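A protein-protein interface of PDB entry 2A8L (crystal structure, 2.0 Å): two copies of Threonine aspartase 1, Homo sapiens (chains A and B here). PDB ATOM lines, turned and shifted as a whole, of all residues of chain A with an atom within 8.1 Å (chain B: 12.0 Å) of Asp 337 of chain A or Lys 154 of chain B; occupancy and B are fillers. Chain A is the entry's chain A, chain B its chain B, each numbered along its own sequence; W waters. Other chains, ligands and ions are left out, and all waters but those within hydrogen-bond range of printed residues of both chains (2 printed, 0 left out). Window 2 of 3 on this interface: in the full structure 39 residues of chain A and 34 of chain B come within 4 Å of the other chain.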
ATOM      1  N   CYS A 293       4.213 -20.902 -17.583  1.00  0.00           N
ATOM      2  CA  CYS A 293       5.500 -20.705 -18.239  1.00  0.00           C
ATOM      3  C   CYS A 293       5.219 -20.338 -19.684  1.00  0.00           C
ATOM      4  O   CYS A 293       4.683 -21.150 -20.436  1.00  0.00           O
ATOM      5  CB  CYS A 293       6.336 -21.985 -18.185  1.00  0.00           C
ATOM      6  SG  CYS A 293       7.944 -21.835 -18.988  1.00  0.00           S
ATOM      7  N   HIS A 296       6.335 -22.730 -22.399  1.00  0.00           N
ATOM      8  CA  HIS A 296       5.535 -23.951 -22.478  1.00  0.00           C
ATOM      9  C   HIS A 296       4.251 -23.712 -23.269  1.00  0.00           C
ATOM     10  O   HIS A 296       3.856 -24.537 -24.091  1.00  0.00           O
ATOM     11  CB  HIS A 296       5.205 -24.464 -21.063  1.00  0.00           C
ATOM     12  CG  HIS A 296       6.416 -24.850 -20.265  1.00  0.00           C
ATOM     13  ND1 HIS A 296       6.340 -25.306 -18.965  1.00  0.00           N
ATOM     14  CD2 HIS A 296       7.732 -24.832 -20.578  1.00  0.00           C
ATOM     15  CE1 HIS A 296       7.557 -25.549 -18.513  1.00  0.00           C
ATOM     16  NE2 HIS A 296       8.422 -25.270 -19.473  1.00  0.00           N
ATOM     17  N   LEU A 333       7.538 -30.198 -25.719  1.00  0.00           N
ATOM     18  CA  LEU A 333       8.031 -29.813 -24.400  1.00  0.00           C
ATOM     19  C   LEU A 333       8.873 -30.922 -23.764  1.00  0.00           C
ATOM     20  O   LEU A 333       9.104 -30.933 -22.557  1.00  0.00           O
ATOM     21  CB  LEU A 333       6.865 -29.427 -23.484  1.00  0.00           C
ATOM     22  CG  LEU A 333       6.052 -28.212 -23.962  1.00  0.00           C
ATOM     23  CD1 LEU A 333       5.048 -27.821 -22.894  1.00  0.00           C
ATOM     24  CD2 LEU A 333       6.984 -27.032 -24.243  1.00  0.00           C
ATOM     25  N   ALA A 334       9.361 -31.841 -24.592  1.00  0.00           N
ATOM     26  CA  ALA A 334      10.180 -32.943 -24.092  1.00  0.00           C
ATOM     27  C   ALA A 334      11.427 -32.411 -23.389  1.00  0.00           C
ATOM     28  O   ALA A 334      12.053 -33.116 -22.593  1.00  0.00           O
ATOM     29  CB  ALA A 334      10.575 -33.869 -25.243  1.00  0.00           C
ATOM     30  N   SER A 335      11.769 -31.155 -23.675  1.00  0.00           N
ATOM     31  CA  SER A 335      12.937 -30.505 -23.090  1.00  0.00           C
ATOM     32  C   SER A 335      12.696 -29.958 -21.686  1.00  0.00           C
ATOM     33  O   SER A 335      13.608 -29.409 -21.070  1.00  0.00           O
ATOM     34  CB  SER A 335      13.391 -29.350 -23.987  1.00  0.00           C
ATOM     35  OG  SER A 335      12.338 -28.405 -24.154  1.00  0.00           O
ATOM     36  N   GLU A 336      11.474 -30.103 -21.186  1.00  0.00           N
ATOM     37  CA  GLU A 336      11.114 -29.595 -19.865  1.00  0.00           C
ATOM     38  C   GLU A 336      11.023 -30.674 -18.795  1.00  0.00           C
ATOM     39  O   GLU A 336      10.692 -31.818 -19.086  1.00  0.00           O
ATOM     40  CB  GLU A 336       9.759 -28.881 -19.940  1.00  0.00           C
ATOM     41  CG  GLU A 336       9.686 -27.836 -21.043  1.00  0.00           C
ATOM     42  CD  GLU A 336      10.812 -26.841 -20.930  1.00  0.00           C
ATOM     43  OE1 GLU A 336      10.932 -26.209 -19.855  1.00  0.00           O
ATOM     44  OE2 GLU A 336      11.584 -26.705 -21.904  1.00  0.00           O
ATOM     45  N   ASP A 337      11.324 -30.290 -17.557  1.00  0.00           N
ATOM     46  CA  ASP A 337      11.225 -31.185 -16.407  1.00  0.00           C
ATOM     47  C   ASP A 337       9.979 -30.695 -15.661  1.00  0.00           C
ATOM     48  O   ASP A 337      10.065 -30.014 -14.631  1.00  0.00           O
ATOM     49  CB  ASP A 337      12.469 -31.069 -15.516  1.00  0.00           C
ATOM     50  CG  ASP A 337      12.382 -31.942 -14.270  1.00  0.00           C
ATOM     51  OD1 ASP A 337      11.585 -32.902 -14.268  1.00  0.00           O
ATOM     52  OD2 ASP A 337      13.123 -31.669 -13.298  1.00  0.00           O
ATOM     53  N   GLY A 338       8.820 -31.036 -16.216  1.00  0.00           N
ATOM     54  CA  GLY A 338       7.554 -30.606 -15.646  1.00  0.00           C
ATOM     55  C   GLY A 338       7.015 -29.495 -16.528  1.00  0.00           C
ATOM     56  O   GLY A 338       7.742 -28.557 -16.853  1.00  0.00           O
ATOM     57  N   VAL A 339       5.755 -29.605 -16.934  1.00  0.00           N
ATOM     58  CA  VAL A 339       5.135 -28.597 -17.795  1.00  0.00           C
ATOM     59  C   VAL A 339       4.150 -27.815 -16.935  1.00  0.00           C
ATOM     60  O   VAL A 339       3.265 -28.390 -16.299  1.00  0.00           O
ATOM     61  CB  VAL A 339       4.437 -29.268 -18.991  1.00  0.00           C
ATOM     62  CG1 VAL A 339       3.662 -28.231 -19.804  1.00  0.00           C
ATOM     63  CG2 VAL A 339       5.494 -29.951 -19.871  1.00  0.00           C
ATOM     64  N   LEU A 340       4.315 -26.498 -16.933  1.00  0.00           N
ATOM     65  CA  LEU A 340       3.523 -25.618 -16.085  1.00  0.00           C
ATOM     66  C   LEU A 340       2.602 -24.649 -16.812  1.00  0.00           C
ATOM     67  O   LEU A 340       3.063 -23.702 -17.442  1.00  0.00           O
ATOM     68  CB  LEU A 340       4.484 -24.841 -15.187  1.00  0.00           C
ATOM     69  CG  LEU A 340       5.359 -25.752 -14.316  1.00  0.00           C
ATOM     70  CD1 LEU A 340       6.475 -24.939 -13.669  1.00  0.00           C
ATOM     71  CD2 LEU A 340       4.488 -26.436 -13.265  1.00  0.00           C
ATOM     72  N   ALA A 402       2.868 -31.756  -9.481  1.00  0.00           N
ATOM     73  CA  ALA A 402       2.863 -30.508 -10.242  1.00  0.00           C
ATOM     74  C   ALA A 402       3.747 -30.650 -11.473  1.00  0.00           C
ATOM     75  O   ALA A 402       4.872 -31.150 -11.383  1.00  0.00           O
ATOM     76  CB  ALA A 402       3.367 -29.360  -9.376  1.00  0.00           C
ATOM     77  N   GLY A 403       3.232 -30.210 -12.617  1.00  0.00           N
ATOM     78  CA  GLY A 403       3.981 -30.298 -13.855  1.00  0.00           C
ATOM     79  C   GLY A 403       3.867 -31.667 -14.498  1.00  0.00           C
ATOM     80  O   GLY A 403       4.355 -31.878 -15.605  1.00  0.00           O
ATOM     81  N   GLN A 404       3.209 -32.595 -13.806  1.00  0.00           N
ATOM     82  CA  GLN A 404       3.044 -33.958 -14.308  1.00  0.00           C
ATOM     83  C   GLN A 404       1.584 -34.377 -14.415  1.00  0.00           C
ATOM     84  O   GLN A 404       1.241 -35.246 -15.212  1.00  0.00           O
ATOM     85  CB  GLN A 404       3.763 -34.958 -13.393  1.00  0.00           C
ATOM     86  CG  GLN A 404       5.273 -34.821 -13.336  1.00  0.00           C
ATOM     87  CD  GLN A 404       5.933 -35.069 -14.676  1.00  0.00           C
ATOM     88  OE1 GLN A 404       5.619 -36.041 -15.368  1.00  0.00           O
ATOM     89  NE2 GLN A 404       6.859 -34.193 -15.048  1.00  0.00           N
ATOM     90  N   ASN B 126      13.010 -27.624 -31.108  1.00  0.00           N
ATOM     91  CA  ASN B 126      13.328 -26.356 -30.461  1.00  0.00           C
ATOM     92  C   ASN B 126      13.152 -25.211 -31.456  1.00  0.00           C
ATOM     93  O   ASN B 126      13.127 -25.431 -32.665  1.00  0.00           O
ATOM     94  CB  ASN B 126      14.753 -26.363 -29.917  1.00  0.00           C
ATOM     95  CG  ASN B 126      14.791 -26.488 -28.410  1.00  0.00           C
ATOM     96  OD1 ASN B 126      14.257 -25.638 -27.695  1.00  0.00           O
ATOM     97  ND2 ASN B 126      15.423 -27.554 -27.914  1.00  0.00           N
ATOM     98  N   LEU B 146      20.106 -18.399 -30.287  1.00  0.00           N
ATOM     99  CA  LEU B 146      19.112 -18.566 -29.231  1.00  0.00           C
ATOM    100  C   LEU B 146      18.701 -20.026 -29.167  1.00  0.00           C
ATOM    101  O   LEU B 146      18.544 -20.603 -28.084  1.00  0.00           O
ATOM    102  CB  LEU B 146      17.876 -17.713 -29.518  1.00  0.00           C
ATOM    103  CG  LEU B 146      17.915 -16.247 -29.096  1.00  0.00           C
ATOM    104  CD1 LEU B 146      16.804 -15.484 -29.815  1.00  0.00           C
ATOM    105  CD2 LEU B 146      17.758 -16.148 -27.575  1.00  0.00           C
ATOM    106  N   LEU B 147      18.516 -20.618 -30.342  1.00  0.00           N
ATOM    107  CA  LEU B 147      18.125 -22.012 -30.440  1.00  0.00           C
ATOM    108  C   LEU B 147      19.227 -22.903 -29.862  1.00  0.00           C
ATOM    109  O   LEU B 147      18.956 -23.769 -29.030  1.00  0.00           O
ATOM    110  CB  LEU B 147      17.846 -22.371 -31.905  1.00  0.00           C
ATOM    111  CG  LEU B 147      17.356 -23.785 -32.236  1.00  0.00           C
ATOM    112  CD1 LEU B 147      16.617 -23.787 -33.566  1.00  0.00           C
ATOM    113  CD2 LEU B 147      18.534 -24.728 -32.288  1.00  0.00           C
ATOM    114  N   CYS B 148      20.463 -22.683 -30.298  1.00  0.00           N
ATOM    115  CA  CYS B 148      21.594 -23.475 -29.820  1.00  0.00           C
ATOM    116  C   CYS B 148      21.746 -23.401 -28.304  1.00  0.00           C
ATOM    117  O   CYS B 148      21.905 -24.425 -27.633  1.00  0.00           O
ATOM    118  CB  CYS B 148      22.886 -23.011 -30.500  1.00  0.00           C
ATOM    119  SG  CYS B 148      22.973 -23.478 -32.248  1.00  0.00           S
ATOM    120  N   GLU B 149      21.697 -22.190 -27.764  1.00  0.00           N
ATOM    121  CA  GLU B 149      21.810 -22.008 -26.327  1.00  0.00           C
ATOM    122  C   GLU B 149      20.678 -22.743 -25.611  1.00  0.00           C
ATOM    123  O   GLU B 149      20.905 -23.439 -24.620  1.00  0.00           O
ATOM    124  CB  GLU B 149      21.760 -20.522 -25.975  1.00  0.00           C
ATOM    125  CG  GLU B 149      22.983 -19.745 -26.418  1.00  0.00           C
ATOM    126  CD  GLU B 149      24.268 -20.333 -25.869  1.00  0.00           C
ATOM    127  OE1 GLU B 149      24.382 -20.475 -24.632  1.00  0.00           O
ATOM    128  OE2 GLU B 149      25.165 -20.657 -26.675  1.00  0.00           O
ATOM    129  N   GLY B 150      19.464 -22.589 -26.129  1.00  0.00           N
ATOM    130  CA  GLY B 150      18.304 -23.226 -25.529  1.00  0.00           C
ATOM    131  C   GLY B 150      18.377 -24.743 -25.489  1.00  0.00           C
ATOM    132  O   GLY B 150      17.896 -25.376 -24.540  1.00  0.00           O
ATOM    133  N   GLN B 151      18.970 -25.327 -26.526  1.00  0.00           N
ATOM    134  CA  GLN B 151      19.103 -26.772 -26.611  1.00  0.00           C
ATOM    135  C   GLN B 151      19.950 -27.298 -25.463  1.00  0.00           C
ATOM    136  O   GLN B 151      19.829 -28.462 -25.074  1.00  0.00           O
ATOM    137  CB  GLN B 151      19.724 -27.156 -27.956  1.00  0.00           C
ATOM    138  CG  GLN B 151      18.800 -26.891 -29.131  1.00  0.00           C
ATOM    139  CD  GLN B 151      19.489 -27.035 -30.475  1.00  0.00           C
ATOM    140  OE1 GLN B 151      20.453 -26.324 -30.770  1.00  0.00           O
ATOM    141  NE2 GLN B 151      18.993 -27.949 -31.299  1.00  0.00           N
ATOM    142  N   LYS B 152      20.800 -26.433 -24.917  1.00  0.00           N
ATOM    143  CA  LYS B 152      21.661 -26.801 -23.800  1.00  0.00           C
ATOM    144  C   LYS B 152      20.838 -27.114 -22.549  1.00  0.00           C
ATOM    145  O   LYS B 152      21.332 -27.746 -21.615  1.00  0.00           O
ATOM    146  CB  LYS B 152      22.664 -25.680 -23.516  1.00  0.00           C
ATOM    147  CG  LYS B 152      23.697 -25.497 -24.622  1.00  0.00           C
ATOM    148  CD  LYS B 152      24.659 -24.354 -24.334  1.00  0.00           C
ATOM    149  CE  LYS B 152      25.607 -24.146 -25.512  1.00  0.00           C
ATOM    150  NZ  LYS B 152      26.583 -23.040 -25.290  1.00  0.00           N
ATOM    151  N   GLY B 153      19.588 -26.660 -22.532  1.00  0.00           N
ATOM    152  CA  GLY B 153      18.705 -26.933 -21.410  1.00  0.00           C
ATOM    153  C   GLY B 153      18.882 -26.112 -20.146  1.00  0.00           C
ATOM    154  O   GLY B 153      19.791 -25.290 -20.040  1.00  0.00           O
ATOM    155  N   LYS B 154      17.998 -26.352 -19.180  1.00  0.00           N
ATOM    156  CA  LYS B 154      18.018 -25.651 -17.896  1.00  0.00           C
ATOM    157  C   LYS B 154      19.278 -25.989 -17.103  1.00  0.00           C
ATOM    158  O   LYS B 154      19.890 -25.111 -16.490  1.00  0.00           O
ATOM    159  CB  LYS B 154      16.803 -26.047 -17.052  1.00  0.00           C
ATOM    160  CG  LYS B 154      15.490 -26.118 -17.801  1.00  0.00           C
ATOM    161  CD  LYS B 154      14.415 -26.760 -16.922  1.00  0.00           C
ATOM    162  CE  LYS B 154      13.130 -27.033 -17.698  1.00  0.00           C
ATOM    163  NZ  LYS B 154      12.111 -27.719 -16.844  1.00  0.00           N
ATOM    164  N   LEU B 155      19.645 -27.269 -17.110  1.00  0.00           N
ATOM    165  CA  LEU B 155      20.822 -27.754 -16.386  1.00  0.00           C
ATOM    166  C   LEU B 155      22.050 -26.869 -16.596  1.00  0.00           C
ATOM    167  O   LEU B 155      22.266 -26.335 -17.686  1.00  0.00           O
ATOM    168  CB  LEU B 155      21.149 -29.186 -16.818  1.00  0.00           C
ATOM    169  CG  LEU B 155      22.227 -29.925 -16.020  1.00  0.00           C
ATOM    170  CD1 LEU B 155      21.768 -30.085 -14.573  1.00  0.00           C
ATOM    171  CD2 LEU B 155      22.487 -31.288 -16.652  1.00  0.00           C
ATOM    172  N   GLY B 158      20.847 -22.231 -16.169  1.00  0.00           N
ATOM    173  CA  GLY B 158      20.275 -22.488 -14.860  1.00  0.00           C
ATOM    174  C   GLY B 158      18.857 -21.964 -14.737  1.00  0.00           C
ATOM    175  O   GLY B 158      18.403 -21.625 -13.647  1.00  0.00           O
ATOM    176  N   ARG B 159      18.158 -21.905 -15.866  1.00  0.00           N
ATOM    177  CA  ARG B 159      16.776 -21.431 -15.922  1.00  0.00           C
ATOM    178  C   ARG B 159      16.221 -21.731 -17.318  1.00  0.00           C
ATOM    179  O   ARG B 159      16.987 -21.956 -18.252  1.00  0.00           O
ATOM    180  CB  ARG B 159      16.725 -19.923 -15.663  1.00  0.00           C
ATOM    181  CG  ARG B 159      15.322 -19.340 -15.686  1.00  0.00           C
ATOM    182  CD  ARG B 159      15.328 -17.841 -15.421  1.00  0.00           C
ATOM    183  NE  ARG B 159      16.098 -17.105 -16.420  1.00  0.00           N
ATOM    184  CZ  ARG B 159      16.154 -15.778 -16.488  1.00  0.00           C
ATOM    185  NH1 ARG B 159      15.485 -15.039 -15.614  1.00  0.00           N
ATOM    186  NH2 ARG B 159      16.880 -15.190 -17.431  1.00  0.00           N
ATOM    187  N   ILE B 160      14.902 -21.745 -17.464  1.00  0.00           N
ATOM    188  CA  ILE B 160      14.308 -22.009 -18.775  1.00  0.00           C
ATOM    189  C   ILE B 160      14.822 -20.975 -19.779  1.00  0.00           C
ATOM    190  O   ILE B 160      14.631 -19.768 -19.598  1.00  0.00           O
ATOM    191  CB  ILE B 160      12.757 -21.937 -18.723  1.00  0.00           C
ATOM    192  CG1 ILE B 160      12.217 -22.976 -17.736  1.00  0.00           C
ATOM    193  CG2 ILE B 160      12.172 -22.199 -20.109  1.00  0.00           C
ATOM    194  CD1 ILE B 160      10.746 -22.818 -17.425  1.00  0.00           C
ATOM    195  N   PRO B 161      15.487 -21.435 -20.851  1.00  0.00           N
ATOM    196  CA  PRO B 161      16.036 -20.560 -21.895  1.00  0.00           C
ATOM    197  C   PRO B 161      14.939 -19.843 -22.688  1.00  0.00           C
ATOM    198  O   PRO B 161      13.864 -20.400 -22.920  1.00  0.00           O
ATOM    199  CB  PRO B 161      16.824 -21.525 -22.789  1.00  0.00           C
ATOM    200  CG  PRO B 161      17.072 -22.722 -21.911  1.00  0.00           C
ATOM    201  CD  PRO B 161      15.792 -22.845 -21.145  1.00  0.00           C
ATOM    202  N   PRO B 162      15.200 -18.595 -23.109  1.00  0.00           N
ATOM    203  CA  PRO B 162      14.245 -17.789 -23.883  1.00  0.00           C
ATOM    204  C   PRO B 162      14.246 -18.262 -25.338  1.00  0.00           C
ATOM    205  O   PRO B 162      15.287 -18.675 -25.856  1.00  0.00           O
ATOM    206  CB  PRO B 162      14.809 -16.369 -23.782  1.00  0.00           C
ATOM    207  CG  PRO B 162      15.828 -16.439 -22.639  1.00  0.00           C
ATOM    208  CD  PRO B 162      16.400 -17.806 -22.781  1.00  0.00           C
ATOM    209  N   CYS B 163      13.094 -18.203 -25.996  1.00  0.00           N
ATOM    210  CA  CYS B 163      13.032 -18.600 -27.395  1.00  0.00           C
ATOM    211  C   CYS B 163      12.642 -17.417 -28.287  1.00  0.00           C
ATOM    212  O   CYS B 163      12.752 -17.491 -29.505  1.00  0.00           O
ATOM    213  CB  CYS B 163      12.049 -19.772 -27.591  1.00  0.00           C
ATOM    214  SG  CYS B 163      10.303 -19.445 -27.257  1.00  0.00           S
HETATM  215  O   HOH W   1      15.615 -27.486 -20.511  1.00  0.00           O
HETATM  216  O   HOH W   2       9.509 -26.907 -15.782  1.00  0.00           O
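The side-chain carboxylate (OE1) of Glu 336 of chain A lies within salt-bridge range of the side-chain amino group (NZ) of Lys 154 of chain B (3.6 Å). N of Asp 337 of chain A lies close to NZ of Lys 154 of chain B (2.8 Å).
The side-chain hydroxyl (OG) of Ser 335 of chain A is in hydrogen-bond range of the side-chain carboxylate (OE2) of Glu 336 of chain A. NE2 of His 296 of chain A sits at hydrogen-bond distance from OE1 of Glu 336 of chain A, 2.7 Å away. N of Leu 340 of chain A is in hydrogen-bond range of ND1 of His 296 of chain A. N of Cys 293 of chain A lies within hydrogen-bond range of O of Leu 340 of chain A, at 3.0 Å. The side-chain sulfur of Cys 293 of chain A sits close to a ring nitrogen (NE2) of His 296 of chain A (3.5 Å).
Among the printed residues, pairs that only touch across the chains: Cys 293 of chain A with Ile 160 of chain B and His 296 of chain A with Ile 160 of chain B.
No residue of chain B comes within 4 Å of Ser 335 of chain A. Glu 336 of chain A touches one residue of chain B. No residue of chain B comes within 4 Å of Gly 338 of chain A. Gly 403 of chain A touches none of the printed residues of chain B. Of the printed residues of chain B, Cys 293 of chain A touches Ile 160 (3.4 Å). Of the printed residues of chain A, Ile 160 of chain B touches Cys 293 (3.4 Å) and His 296 (3.95 Å). Of the printed residues of chain B, His 296 of chain A touches Ile 160 (3.95 Å). The nearest residue of chain B that does not touch Asp 337 of chain A is Ile 160 of chain B (7.4 Å). The nearest residue of chain A that does not touch Lys 154 of chain B is Ser 335 of chain A (4.2 Å). The nearest printed residue of chain B that does not touch His 296 of chain A is Lys 154 of chain B (5.1 Å).
Printed residues of chain B that touch a printed residue of chain A: Lys 154 and Ile 160. Hydrophobic or aromatic side chains of chain B within 4 Å of the printed part of chain A: Ile 160. Hydrophobic or aromatic side chains of chain A that line the printed part of chain B: His 296. Along chain A the printed residues that touch a printed residue of chain B span positions 293 to 337. Among the printed residues, Asp or Glu carboxylates within 4 Å of a Lys or Arg side-chain nitrogen of the other chain: Glu 336 of chain A with Lys 154 of chain B.
No position is printed for both chains. Of the 4 pairs that touch across the chains among the printed residues, none has its exchanged pair printed and touching as well.
Water W2 lies within hydrogen-bond range of O of Gly 338 of chain A (2.6 Å), NZ of Lys 154 of chain B (2.9 Å) and O of Asp 337 of chain A (3.4 Å). Water W1 bridges the backbone carbonyl oxygen of Ser 335 of chain A and the backbone NH of Lys 154 of chain B.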
